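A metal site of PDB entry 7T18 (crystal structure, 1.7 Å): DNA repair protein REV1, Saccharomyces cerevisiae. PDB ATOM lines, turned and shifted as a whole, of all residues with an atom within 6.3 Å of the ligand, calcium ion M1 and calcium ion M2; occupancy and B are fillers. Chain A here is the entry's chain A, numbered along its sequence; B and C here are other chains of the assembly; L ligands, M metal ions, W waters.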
ATOM      1  N   ARG A  29       7.241  -7.541 -27.343  1.00  0.00           N
ATOM      2  CA  ARG A  29       8.584  -7.818 -26.832  1.00  0.00           C
ATOM      3  C   ARG A  29       9.629  -6.957 -27.528  1.00  0.00           C
ATOM      4  O   ARG A  29      10.580  -6.486 -26.891  1.00  0.00           O
ATOM      5  CB  ARG A  29       8.932  -9.300 -26.995  1.00  0.00           C
ATOM      6  CG  ARG A  29       9.189  -9.740 -28.449  1.00  0.00           C
ATOM      7  CD  ARG A  29       9.204 -11.240 -28.540  1.00  0.00           C
ATOM      8  NE  ARG A  29      10.052 -11.741 -29.612  1.00  0.00           N
ATOM      9  CZ  ARG A  29       9.652 -11.918 -30.866  1.00  0.00           C
ATOM     10  NH1 ARG A  29       8.411 -11.601 -31.201  1.00  0.00           N
ATOM     11  NH2 ARG A  29      10.490 -12.404 -31.778  1.00  0.00           N
ATOM     12  N   LEU A  30       9.473  -6.733 -28.832  1.00  0.00           N
ATOM     13  CA  LEU A  30      10.493  -5.994 -29.561  1.00  0.00           C
ATOM     14  C   LEU A  30      10.473  -4.518 -29.176  1.00  0.00           C
ATOM     15  O   LEU A  30      11.522  -3.868 -29.117  1.00  0.00           O
ATOM     16  CB  LEU A  30      10.332  -6.203 -31.059  1.00  0.00           C
ATOM     17  CG  LEU A  30      10.629  -7.643 -31.533  1.00  0.00           C
ATOM     18  CD1 LEU A  30      10.227  -7.849 -32.985  1.00  0.00           C
ATOM     19  CD2 LEU A  30      12.076  -7.959 -31.350  1.00  0.00           C
ATOM     20  N   LEU A  33      12.362  -4.485 -25.931  1.00  0.00           N
ATOM     21  CA  LEU A  33      13.809  -4.691 -26.230  1.00  0.00           C
ATOM     22  C   LEU A  33      14.469  -3.349 -26.573  1.00  0.00           C
ATOM     23  O   LEU A  33      15.533  -3.053 -26.011  1.00  0.00           O
ATOM     24  CB  LEU A  33      13.943  -5.682 -27.387  1.00  0.00           C
ATOM     25  CG  LEU A  33      14.803  -6.910 -27.108  1.00  0.00           C
ATOM     26  CD1 LEU A  33      15.354  -7.498 -28.404  1.00  0.00           C
ATOM     27  CD2 LEU A  33      15.953  -6.566 -26.158  1.00  0.00           C
ATOM     28  N   TRP A  36      14.085  -0.670 -23.438  1.00  0.00           N
ATOM     29  CA  TRP A  36      15.064  -0.998 -22.419  1.00  0.00           C
ATOM     30  C   TRP A  36      16.465  -0.557 -22.811  1.00  0.00           C
ATOM     31  O   TRP A  36      17.196   0.013 -21.999  1.00  0.00           O
ATOM     32  CB  TRP A  36      15.071  -2.502 -22.177  1.00  0.00           C
ATOM     33  CG  TRP A  36      13.883  -3.028 -21.500  1.00  0.00           C
ATOM     34  CD1 TRP A  36      13.115  -2.413 -20.555  1.00  0.00           C
ATOM     35  CD2 TRP A  36      13.320  -4.328 -21.687  1.00  0.00           C
ATOM     36  NE1 TRP A  36      12.105  -3.253 -20.148  1.00  0.00           N
ATOM     37  CE2 TRP A  36      12.221  -4.439 -20.829  1.00  0.00           C
ATOM     38  CE3 TRP A  36      13.666  -5.429 -22.493  1.00  0.00           C
ATOM     39  CZ2 TRP A  36      11.446  -5.595 -20.758  1.00  0.00           C
ATOM     40  CZ3 TRP A  36      12.904  -6.567 -22.421  1.00  0.00           C
ATOM     41  CH2 TRP A  36      11.800  -6.637 -21.564  1.00  0.00           C
ATOM     42  N   ASP A  67      25.991 -12.583 -20.320  1.00  0.00           N
ATOM     43  CA  ASP A  67      24.665 -12.618 -20.925  1.00  0.00           C
ATOM     44  C   ASP A  67      23.811 -13.673 -20.222  1.00  0.00           C
ATOM     45  O   ASP A  67      24.291 -14.780 -19.951  1.00  0.00           O
ATOM     46  CB  ASP A  67      24.787 -12.910 -22.434  1.00  0.00           C
ATOM     47  CG  ASP A  67      23.454 -13.208 -23.092  1.00  0.00           C
ATOM     48  OD1 ASP A  67      23.075 -14.385 -23.142  1.00  0.00           O
ATOM     49  OD2 ASP A  67      22.790 -12.257 -23.542  1.00  0.00           O
ATOM     50  N   PHE A  68      22.560 -13.325 -19.903  1.00  0.00           N
ATOM     51  CA  PHE A  68      21.634 -14.288 -19.301  1.00  0.00           C
ATOM     52  C   PHE A  68      21.340 -15.434 -20.274  1.00  0.00           C
ATOM     53  O   PHE A  68      21.040 -15.203 -21.450  1.00  0.00           O
ATOM     54  CB  PHE A  68      20.283 -13.624 -18.987  1.00  0.00           C
ATOM     55  CG  PHE A  68      20.221 -12.796 -17.727  1.00  0.00           C
ATOM     56  CD1 PHE A  68      20.787 -11.539 -17.670  1.00  0.00           C
ATOM     57  CD2 PHE A  68      19.474 -13.234 -16.646  1.00  0.00           C
ATOM     58  CE1 PHE A  68      20.663 -10.732 -16.536  1.00  0.00           C
ATOM     59  CE2 PHE A  68      19.327 -12.443 -15.505  1.00  0.00           C
ATOM     60  CZ  PHE A  68      19.930 -11.202 -15.441  1.00  0.00           C
ATOM     61  N   ASP A  69      21.338 -16.647 -19.758  1.00  0.00           N
ATOM     62  CA  ASP A  69      20.874 -17.797 -20.552  1.00  0.00           C
ATOM     63  C   ASP A  69      19.343 -17.721 -20.658  1.00  0.00           C
ATOM     64  O   ASP A  69      18.726 -17.572 -19.649  1.00  0.00           O
ATOM     65  CB  ASP A  69      21.244 -19.125 -19.875  1.00  0.00           C
ATOM     66  CG  ASP A  69      22.733 -19.221 -19.619  1.00  0.00           C
ATOM     67  OD1 ASP A  69      23.463 -18.912 -20.520  1.00  0.00           O
ATOM     68  OD2 ASP A  69      23.094 -19.563 -18.542  1.00  0.00           O
ATOM     69  N   CYS A  70      18.829 -18.009 -21.840  1.00  0.00           N
ATOM     70  CA  CYS A  70      17.403 -17.958 -22.240  1.00  0.00           C
ATOM     71  C   CYS A  70      16.628 -16.982 -21.352  1.00  0.00           C
ATOM     72  O   CYS A  70      15.794 -17.404 -20.638  1.00  0.00           O
ATOM     73  CB  CYS A  70      16.781 -19.345 -22.287  1.00  0.00           C
ATOM     74  SG  CYS A  70      17.115 -20.346 -20.811  1.00  0.00           S
ATOM     75  N   PHE A  71      16.981 -15.696 -21.464  1.00  0.00           N
ATOM     76  CA  PHE A  71      16.506 -14.729 -20.483  1.00  0.00           C
ATOM     77  C   PHE A  71      15.006 -14.768 -20.183  1.00  0.00           C
ATOM     78  O   PHE A  71      14.597 -14.978 -19.042  1.00  0.00           O
ATOM     79  CB  PHE A  71      16.913 -13.338 -20.958  1.00  0.00           C
ATOM     80  CG  PHE A  71      16.560 -12.240 -20.019  1.00  0.00           C
ATOM     81  CD1 PHE A  71      16.909 -12.314 -18.690  1.00  0.00           C
ATOM     82  CD2 PHE A  71      15.854 -11.126 -20.474  1.00  0.00           C
ATOM     83  CE1 PHE A  71      16.593 -11.296 -17.816  1.00  0.00           C
ATOM     84  CE2 PHE A  71      15.513 -10.108 -19.597  1.00  0.00           C
ATOM     85  CZ  PHE A  71      15.890 -10.189 -18.277  1.00  0.00           C
ATOM     86  N   PHE A  72      14.152 -14.541 -21.195  1.00  0.00           N
ATOM     87  CA  PHE A  72      12.716 -14.498 -20.909  1.00  0.00           C
ATOM     88  C   PHE A  72      12.226 -15.836 -20.377  1.00  0.00           C
ATOM     89  O   PHE A  72      11.343 -15.873 -19.508  1.00  0.00           O
ATOM     90  CB  PHE A  72      11.904 -14.145 -22.148  1.00  0.00           C
ATOM     91  CG  PHE A  72      11.899 -12.687 -22.532  1.00  0.00           C
ATOM     92  CD1 PHE A  72      12.806 -11.768 -22.027  1.00  0.00           C
ATOM     93  CD2 PHE A  72      10.945 -12.246 -23.458  1.00  0.00           C
ATOM     94  CE1 PHE A  72      12.773 -10.441 -22.434  1.00  0.00           C
ATOM     95  CE2 PHE A  72      10.895 -10.913 -23.864  1.00  0.00           C
ATOM     96  CZ  PHE A  72      11.831 -10.019 -23.364  1.00  0.00           C
ATOM     97  N   ALA A  73      12.728 -16.952 -20.914  1.00  0.00           N
ATOM     98  CA  ALA A  73      12.247 -18.255 -20.436  1.00  0.00           C
ATOM     99  C   ALA A  73      12.642 -18.482 -18.981  1.00  0.00           C
ATOM    100  O   ALA A  73      11.832 -18.956 -18.190  1.00  0.00           O
ATOM    101  CB  ALA A  73      12.775 -19.383 -21.326  1.00  0.00           C
ATOM    102  N   ALA A 106       9.499 -16.031 -27.977  1.00  0.00           N
ATOM    103  CA  ALA A 106      10.437 -14.994 -27.549  1.00  0.00           C
ATOM    104  C   ALA A 106      11.712 -15.601 -26.993  1.00  0.00           C
ATOM    105  O   ALA A 106      12.812 -15.080 -27.232  1.00  0.00           O
ATOM    106  CB  ALA A 106       9.759 -14.093 -26.518  1.00  0.00           C
ATOM    107  N   SER A 107      11.581 -16.693 -26.247  1.00  0.00           N
ATOM    108  CA  SER A 107      12.704 -17.379 -25.629  1.00  0.00           C
ATOM    109  C   SER A 107      12.288 -18.814 -25.407  1.00  0.00           C
ATOM    110  O   SER A 107      11.126 -19.097 -25.108  1.00  0.00           O
ATOM    111  CB  SER A 107      13.077 -16.720 -24.292  1.00  0.00           C
ATOM    112  OG  SER A 107      14.277 -17.260 -23.742  1.00  0.00           O
ATOM    113  N   CYS A 108      13.240 -19.721 -25.564  1.00  0.00           N
ATOM    114  CA  CYS A 108      12.980 -21.111 -25.227  1.00  0.00           C
ATOM    115  C   CYS A 108      14.159 -21.610 -24.405  1.00  0.00           C
ATOM    116  O   CYS A 108      15.283 -21.152 -24.588  1.00  0.00           O
ATOM    117  CB  CYS A 108      12.796 -21.979 -26.473  1.00  0.00           C
ATOM    118  SG  CYS A 108      14.175 -21.860 -27.635  1.00  0.00           S
ATOM    119  N   TYR A 110      16.831 -24.552 -22.786  1.00  0.00           N
ATOM    120  CA  TYR A 110      17.772 -25.390 -23.516  1.00  0.00           C
ATOM    121  C   TYR A 110      17.260 -26.810 -23.695  1.00  0.00           C
ATOM    122  O   TYR A 110      17.742 -27.518 -24.586  1.00  0.00           O
ATOM    123  CB  TYR A 110      19.151 -25.336 -22.820  1.00  0.00           C
ATOM    124  CG  TYR A 110      19.888 -24.079 -23.233  1.00  0.00           C
ATOM    125  CD1 TYR A 110      19.537 -22.843 -22.709  1.00  0.00           C
ATOM    126  CD2 TYR A 110      20.902 -24.116 -24.176  1.00  0.00           C
ATOM    127  CE1 TYR A 110      20.183 -21.672 -23.119  1.00  0.00           C
ATOM    128  CE2 TYR A 110      21.570 -22.954 -24.579  1.00  0.00           C
ATOM    129  CZ  TYR A 110      21.198 -21.742 -24.053  1.00  0.00           C
ATOM    130  OH  TYR A 110      21.834 -20.586 -24.451  1.00  0.00           O
ATOM    131  N   ARG A 113      15.599 -26.373 -26.918  1.00  0.00           N
ATOM    132  CA  ARG A 113      16.607 -26.249 -27.958  1.00  0.00           C
ATOM    133  C   ARG A 113      17.241 -27.577 -28.314  1.00  0.00           C
ATOM    134  O   ARG A 113      17.741 -27.732 -29.430  1.00  0.00           O
ATOM    135  CB  ARG A 113      17.686 -25.247 -27.525  1.00  0.00           C
ATOM    136  CG  ARG A 113      17.147 -23.826 -27.344  1.00  0.00           C
ATOM    137  CD  ARG A 113      18.217 -22.836 -26.885  1.00  0.00           C
ATOM    138  NE  ARG A 113      17.587 -21.604 -26.411  1.00  0.00           N
ATOM    139  CZ  ARG A 113      18.177 -20.418 -26.354  1.00  0.00           C
ATOM    140  NH1 ARG A 113      19.442 -20.285 -26.748  1.00  0.00           N
ATOM    141  NH2 ARG A 113      17.498 -19.361 -25.911  1.00  0.00           N
ATOM    142  N   ASN A 119      14.712 -19.505 -30.631  1.00  0.00           N
ATOM    143  CA  ASN A 119      14.047 -18.219 -30.473  1.00  0.00           C
ATOM    144  C   ASN A 119      13.586 -17.716 -31.832  1.00  0.00           C
ATOM    145  O   ASN A 119      14.303 -17.825 -32.835  1.00  0.00           O
ATOM    146  CB  ASN A 119      14.994 -17.183 -29.855  1.00  0.00           C
ATOM    147  CG  ASN A 119      15.292 -17.447 -28.392  1.00  0.00           C
ATOM    148  OD1 ASN A 119      14.815 -18.413 -27.820  1.00  0.00           O
ATOM    149  ND2 ASN A 119      16.094 -16.567 -27.783  1.00  0.00           N
ATOM    150  N   TYR A 141       4.509 -13.810 -20.930  1.00  0.00           N
ATOM    151  CA  TYR A 141       5.499 -12.795 -20.629  1.00  0.00           C
ATOM    152  C   TYR A 141       5.300 -12.213 -19.232  1.00  0.00           C
ATOM    153  O   TYR A 141       4.181 -12.078 -18.732  1.00  0.00           O
ATOM    154  CB  TYR A 141       5.414 -11.655 -21.637  1.00  0.00           C
ATOM    155  CG  TYR A 141       5.733 -12.009 -23.062  1.00  0.00           C
ATOM    156  CD1 TYR A 141       4.749 -12.508 -23.916  1.00  0.00           C
ATOM    157  CD2 TYR A 141       7.009 -11.822 -23.581  1.00  0.00           C
ATOM    158  CE1 TYR A 141       5.028 -12.815 -25.236  1.00  0.00           C
ATOM    159  CE2 TYR A 141       7.296 -12.123 -24.904  1.00  0.00           C
ATOM    160  CZ  TYR A 141       6.304 -12.597 -25.726  1.00  0.00           C
ATOM    161  OH  TYR A 141       6.607 -12.887 -27.054  1.00  0.00           O
ATOM    162  N   ILE A 169      24.710  -3.692 -23.269  1.00  0.00           N
ATOM    163  CA  ILE A 169      24.386  -4.153 -24.603  1.00  0.00           C
ATOM    164  C   ILE A 169      22.880  -4.316 -24.771  1.00  0.00           C
ATOM    165  O   ILE A 169      22.317  -3.933 -25.794  1.00  0.00           O
ATOM    166  CB  ILE A 169      25.109  -5.479 -24.913  1.00  0.00           C
ATOM    167  CG1 ILE A 169      26.620  -5.305 -24.822  1.00  0.00           C
ATOM    168  CG2 ILE A 169      24.698  -6.010 -26.277  1.00  0.00           C
ATOM    169  CD1 ILE A 169      27.179  -4.363 -25.883  1.00  0.00           C
ATOM    170  N   SER A 170      22.228  -4.879 -23.753  1.00  0.00           N
ATOM    171  CA  SER A 170      20.792  -5.090 -23.809  1.00  0.00           C
ATOM    172  C   SER A 170      20.292  -5.338 -22.389  1.00  0.00           C
ATOM    173  O   SER A 170      21.054  -5.257 -21.418  1.00  0.00           O
ATOM    174  CB  SER A 170      20.447  -6.265 -24.724  1.00  0.00           C
ATOM    175  OG  SER A 170      20.547  -7.462 -24.005  1.00  0.00           O
ATOM    176  N   ILE A 171      18.997  -5.606 -22.281  1.00  0.00           N
ATOM    177  CA  ILE A 171      18.351  -5.886 -21.002  1.00  0.00           C
ATOM    178  C   ILE A 171      19.086  -7.000 -20.250  1.00  0.00           C
ATOM    179  O   ILE A 171      19.154  -6.987 -19.014  1.00  0.00           O
ATOM    180  CB  ILE A 171      16.864  -6.235 -21.252  1.00  0.00           C
ATOM    181  CG1 ILE A 171      16.117  -6.424 -19.924  1.00  0.00           C
ATOM    182  CG2 ILE A 171      16.712  -7.499 -22.120  1.00  0.00           C
ATOM    183  CD1 ILE A 171      15.753  -5.117 -19.276  1.00  0.00           C
ATOM    184  N   ASP A 172      19.660  -7.963 -20.981  1.00  0.00           N
ATOM    185  CA  ASP A 172      20.251  -9.139 -20.348  1.00  0.00           C
ATOM    186  C   ASP A 172      21.729  -9.337 -20.690  1.00  0.00           C
ATOM    187  O   ASP A 172      22.252 -10.444 -20.527  1.00  0.00           O
ATOM    188  CB  ASP A 172      19.457 -10.407 -20.717  1.00  0.00           C
ATOM    189  CG  ASP A 172      19.825 -10.948 -22.088  1.00  0.00           C
ATOM    190  OD1 ASP A 172      20.114 -10.143 -22.984  1.00  0.00           O
ATOM    191  OD2 ASP A 172      19.835 -12.180 -22.274  1.00  0.00           O
ATOM    192  N   GLU A 173      22.429  -8.291 -21.135  1.00  0.00           N
ATOM    193  CA  GLU A 173      23.756  -8.525 -21.683  1.00  0.00           C
ATOM    194  C   GLU A 173      24.610  -7.281 -21.500  1.00  0.00           C
ATOM    195  O   GLU A 173      24.150  -6.171 -21.782  1.00  0.00           O
ATOM    196  CB  GLU A 173      23.663  -8.894 -23.166  1.00  0.00           C
ATOM    197  CG  GLU A 173      24.973  -9.212 -23.838  1.00  0.00           C
ATOM    198  CD  GLU A 173      24.756  -9.592 -25.294  1.00  0.00           C
ATOM    199  OE1 GLU A 173      25.745  -9.693 -26.056  1.00  0.00           O
ATOM    200  OE2 GLU A 173      23.581  -9.792 -25.667  1.00  0.00           O
ATOM    201  N   LYS A 230      27.836 -21.247 -23.433  1.00  0.00           N
ATOM    202  CA  LYS A 230      26.441 -21.485 -23.084  1.00  0.00           C
ATOM    203  C   LYS A 230      26.092 -22.969 -23.130  1.00  0.00           C
ATOM    204  O   LYS A 230      26.655 -23.719 -23.941  1.00  0.00           O
ATOM    205  CB  LYS A 230      25.522 -20.720 -24.050  1.00  0.00           C
ATOM    206  CG  LYS A 230      25.454 -19.229 -23.743  1.00  0.00           C
ATOM    207  CD  LYS A 230      24.646 -18.470 -24.773  1.00  0.00           C
ATOM    208  CE  LYS A 230      24.265 -17.085 -24.245  1.00  0.00           C
ATOM    209  NZ  LYS A 230      23.529 -17.134 -22.930  1.00  0.00           N
ATOM    210  P    DG B  12      24.588  -6.810 -30.325  1.00  0.00           P
ATOM    211  OP1  DG B  12      25.520  -5.721 -29.880  1.00  0.00           O
ATOM    212  OP2  DG B  12      25.080  -8.159 -30.451  1.00  0.00           O
ATOM    213  O5'  DG B  12      23.397  -6.859 -29.293  1.00  0.00           O
ATOM    214  C5'  DG B  12      22.804  -8.074 -28.851  1.00  0.00           C
ATOM    215  C4'  DG B  12      21.420  -7.709 -28.393  1.00  0.00           C
ATOM    216  O4'  DG B  12      20.799  -7.034 -29.502  1.00  0.00           O
ATOM    217  C3'  DG B  12      20.479  -8.842 -28.027  1.00  0.00           C
ATOM    218  O3'  DG B  12      20.540  -9.142 -26.633  1.00  0.00           O
ATOM    219  C2'  DG B  12      19.131  -8.248 -28.357  1.00  0.00           C
ATOM    220  C1'  DG B  12      19.435  -7.148 -29.385  1.00  0.00           C
ATOM    221  N9   DG B  12      18.874  -7.445 -30.698  1.00  0.00           N
ATOM    222  C8   DG B  12      18.986  -8.598 -31.438  1.00  0.00           C
ATOM    223  N7   DG B  12      18.192  -8.621 -32.463  1.00  0.00           N
ATOM    224  C5   DG B  12      17.452  -7.460 -32.345  1.00  0.00           C
ATOM    225  C6   DG B  12      16.403  -6.958 -33.148  1.00  0.00           C
ATOM    226  O6   DG B  12      15.935  -7.422 -34.175  1.00  0.00           O
ATOM    227  N1   DG B  12      15.945  -5.722 -32.683  1.00  0.00           N
ATOM    228  C2   DG B  12      16.398  -5.103 -31.551  1.00  0.00           C
ATOM    229  N2   DG B  12      15.809  -3.959 -31.230  1.00  0.00           N
ATOM    230  N3   DG B  12      17.367  -5.565 -30.791  1.00  0.00           N
ATOM    231  C4   DG B  12      17.870  -6.723 -31.260  1.00  0.00           C
ATOM    232  P    DC C   5       7.118  -4.066 -35.595  1.00  0.00           P
ATOM    233  OP1  DC C   5       5.672  -3.786 -35.534  1.00  0.00           O
ATOM    234  OP2  DC C   5       7.860  -3.761 -36.834  1.00  0.00           O
ATOM    235  O5'  DC C   5       7.912  -3.311 -34.440  1.00  0.00           O
ATOM    236  C5'  DC C   5       7.446  -3.376 -33.106  1.00  0.00           C
ATOM    237  C4'  DC C   5       8.417  -2.712 -32.158  1.00  0.00           C
ATOM    238  O4'  DC C   5       9.647  -3.469 -32.096  1.00  0.00           O
ATOM    239  C3'  DC C   5       8.840  -1.305 -32.544  1.00  0.00           C
ATOM    240  O3'  DC C   5       9.110  -0.604 -31.364  1.00  0.00           O
ATOM    241  C2'  DC C   5      10.119  -1.533 -33.358  1.00  0.00           C
ATOM    242  C1'  DC C   5      10.731  -2.715 -32.624  1.00  0.00           C
ATOM    243  N1   DC C   5      11.517  -3.651 -33.471  1.00  0.00           N
ATOM    244  C2   DC C   5      12.836  -3.934 -33.132  1.00  0.00           C
ATOM    245  O2   DC C   5      13.341  -3.352 -32.160  1.00  0.00           O
ATOM    246  N3   DC C   5      13.515  -4.844 -33.853  1.00  0.00           N
ATOM    247  C4   DC C   5      12.932  -5.447 -34.876  1.00  0.00           C
ATOM    248  N4   DC C   5      13.640  -6.330 -35.563  1.00  0.00           N
ATOM    249  C5   DC C   5      11.572  -5.189 -35.239  1.00  0.00           C
ATOM    250  C6   DC C   5      10.913  -4.298 -34.501  1.00  0.00           C
HETATM  251  P1  LIG L   1      18.966 -13.233 -26.451  1.00  0.00           P
HETATM  252  O1  LIG L   1      20.092 -13.021 -25.553  1.00  0.00           O
HETATM  253  O2  LIG L   1      19.276 -13.165 -27.875  1.00  0.00           O
HETATM  254  O3  LIG L   1      18.318 -14.669 -26.204  1.00  0.00           O
HETATM  255  P2  LIG L   1      18.089 -15.608 -24.931  1.00  0.00           P
HETATM  256  O4  LIG L   1      18.679 -14.947 -23.792  1.00  0.00           O
HETATM  257  O5  LIG L   1      16.591 -15.987 -24.835  1.00  0.00           O
HETATM  258  O6  LIG L   1      18.903 -16.937 -25.238  1.00  0.00           O
HETATM  259  P3  LIG L   1      20.476 -17.201 -25.181  1.00  0.00           P
HETATM  260  O7  LIG L   1      21.126 -15.872 -24.932  1.00  0.00           O
HETATM  261  O8  LIG L   1      20.754 -18.193 -24.029  1.00  0.00           O
HETATM  262  O9  LIG L   1      20.855 -17.838 -26.530  1.00  0.00           O
HETATM  263  O10 LIG L   1      17.822 -12.196 -26.124  1.00  0.00           O
HETATM  264  C1  LIG L   1      17.488 -11.821 -24.782  1.00  0.00           C
HETATM  265  C2  LIG L   1      15.991 -11.756 -24.640  1.00  0.00           C
HETATM  266  O11 LIG L   1      15.511 -10.705 -25.493  1.00  0.00           O
HETATM  267  C3  LIG L   1      15.263 -13.013 -25.102  1.00  0.00           C
HETATM  268  O12 LIG L   1      15.073 -13.934 -24.029  1.00  0.00           O
HETATM  269  C4  LIG L   1      13.954 -12.492 -25.639  1.00  0.00           C
HETATM  270  C5  LIG L   1      14.287 -11.084 -26.108  1.00  0.00           C
HETATM  271  N1  LIG L   1      14.461 -10.998 -27.562  1.00  0.00           N
HETATM  272  C6  LIG L   1      13.324 -10.773 -28.344  1.00  0.00           C
HETATM  273  O13 LIG L   1      12.234 -10.649 -27.817  1.00  0.00           O
HETATM  274  N2  LIG L   1      13.454 -10.684 -29.727  1.00  0.00           N
HETATM  275  C7  LIG L   1      14.682 -10.876 -30.213  1.00  0.00           C
HETATM  276  O14 LIG L   1      14.768 -10.816 -31.436  1.00  0.00           O
HETATM  277  C8  LIG L   1      15.865 -11.119 -29.484  1.00  0.00           C
HETATM  278  C9  LIG L   1      17.216 -11.304 -30.128  1.00  0.00           C
HETATM  279  C10 LIG L   1      15.765 -11.229 -28.093  1.00  0.00           C
HETATM  280 CA    CA M   1      20.790 -13.998 -23.457  1.00  0.00          CA
HETATM  281 CA    CA M   2      21.305 -10.821 -24.998  1.00  0.00          CA
HETATM  282  O   HOH W   1      14.389 -13.951 -32.147  1.00  0.00           O
HETATM  283  O   HOH W   2      19.502 -17.316 -28.970  1.00  0.00           O
HETATM  284  O   HOH W   3      15.008 -10.015 -34.431  1.00  0.00           O
HETATM  285  O   HOH W   4      12.529 -13.338 -29.293  1.00  0.00           O
HETATM  286  O   HOH W   5      17.640 -14.724 -29.388  1.00  0.00           O
HETATM  287  O   HOH W   6      23.265 -18.121 -27.785  1.00  0.00           O
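The guanidinium group (NE) of Arg 113 lies within hydrogen-bond range of the backbone carbonyl oxygen (O) of Cys 108 (3.0 Å). The side-chain hydroxyl (OG) of Ser 107 is in hydrogen-bond range of the backbone NH (N) of Ala 73. O3' of DG 12 of chain B sits close to the side-chain hydroxyl (OG) of Ser 170, at 3.1 Å. N of Asp 172 sits close to OG of Ser 170 (3.2 Å). OG of Ser 107 sits close to O of Cys 70, 3.5 Å away. OD1 of Asp 67 lies close to NZ of Lys 230, 2.8 Å away. The backbone carbonyl oxygen (O) of Phe 68 sits close to the side-chain amino group (NZ) of Lys 230 (3.5 Å). O2 of DC 5 of chain C sits close to N2 of DG 12 of chain B (2.7 Å).
Residues that only touch calcium ion M2: Ser 170 (3.6 Å).
Within 4 Å of calcium ion M1: Asp 67, Phe 68 and Asp 172.
NZ of Lys 230 lies within salt-bridge range of O8 of the ligand (3.2 Å). NH1 of Arg 113 is in salt-bridge range of O9 of the ligand (2.8 Å). An oxygen (O13) of the ligand is in hydrogen-bond range of the guanidinium group (NE) of Arg 29 (3.0 Å). N of Phe 72 lies within hydrogen-bond range of O12 of the ligand (3.0 Å). OH of Tyr 110 lies within hydrogen-bond range of O8 of the ligand, at 2.7 Å. The backbone NH (N) of Phe 71 is in hydrogen-bond range of an oxygen (O5) of the ligand (3.4 Å). OG of Ser 107 lies within hydrogen-bond range of O5 of the ligand, 2.9 Å away. ND2 of Asn 119 sits at hydrogen-bond distance from O5 of the ligand (3.0 Å). The backbone NH of Cys 70 sits at hydrogen-bond distance from an oxygen (O8) of the ligand, at 2.9 Å.
Water W5 lies within hydrogen-bond range of an oxygen (O2) of the ligand and the side-chain amide nitrogen (ND2) of Asn 119. Water W4 lies within hydrogen-bond range of the backbone carbonyl oxygen of Ala 106 (2.7 Å), a nitrogen (N2) of the ligand (2.8 Å) and the guanidinium group of Arg 29 (3.0 Å). Water W3 bridges O6 of DG 12 of chain B and O14 of the ligand.
Calcium ion M2 is bound by the side-chain carboxylate (OD1) of Asp 172, O3' of DG 12 of chain B, the side-chain carboxylate (OD2) of Asp 67, an oxygen (O1) of the ligand and the side-chain carboxylate (OE2) of Glu 173. Calcium ion M2 has five donor atoms within binding distance.
Leu 30 touches the ligand. Leu 33 touches the ligand (CD1 to N1, 3.7 Å). Asp 69 touches the ligand (CA to O8, 3.5 Å). Ala 106 touches the ligand (O to C4, 3.2 Å). Hydrophobic or aromatic side chains that line the ligand: Leu 30, Leu 33, Phe 71, Phe 72 and Tyr 110. Within 4 Å of the ligand: Arg 29, Leu 30, Leu 33, Asp 67, Phe 68, Asp 69, Cys 70, Phe 71, Phe 72, Ala 106, Ser 107, Tyr 110, Arg 113, Asn 119, Asp 172, Lys 230 and DG 12 of chain B. The nearest printed residue that does not touch the ligand is Glu 173 (4.8 Å).
Calcium ion M1 is bound by OD1 of Asp 67, at 2.3 Å. An oxygen (O4) of the ligand is bound to calcium ion M1 (2.3 Å). Calcium ion M1 is bound by O of Phe 68 (2.4 Å). OD2 of Asp 172 binds calcium ion M1. O7 of the ligand binds calcium ion M1, at 2.4 Å. O1 of the ligand binds calcium ion M1 (2.4 Å). Calcium ion M1 is bound by the side-chain carboxylate (OD2) of Asp 67, 2.7 Å away. Calcium ion M1 has seven donor atoms within binding distance.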
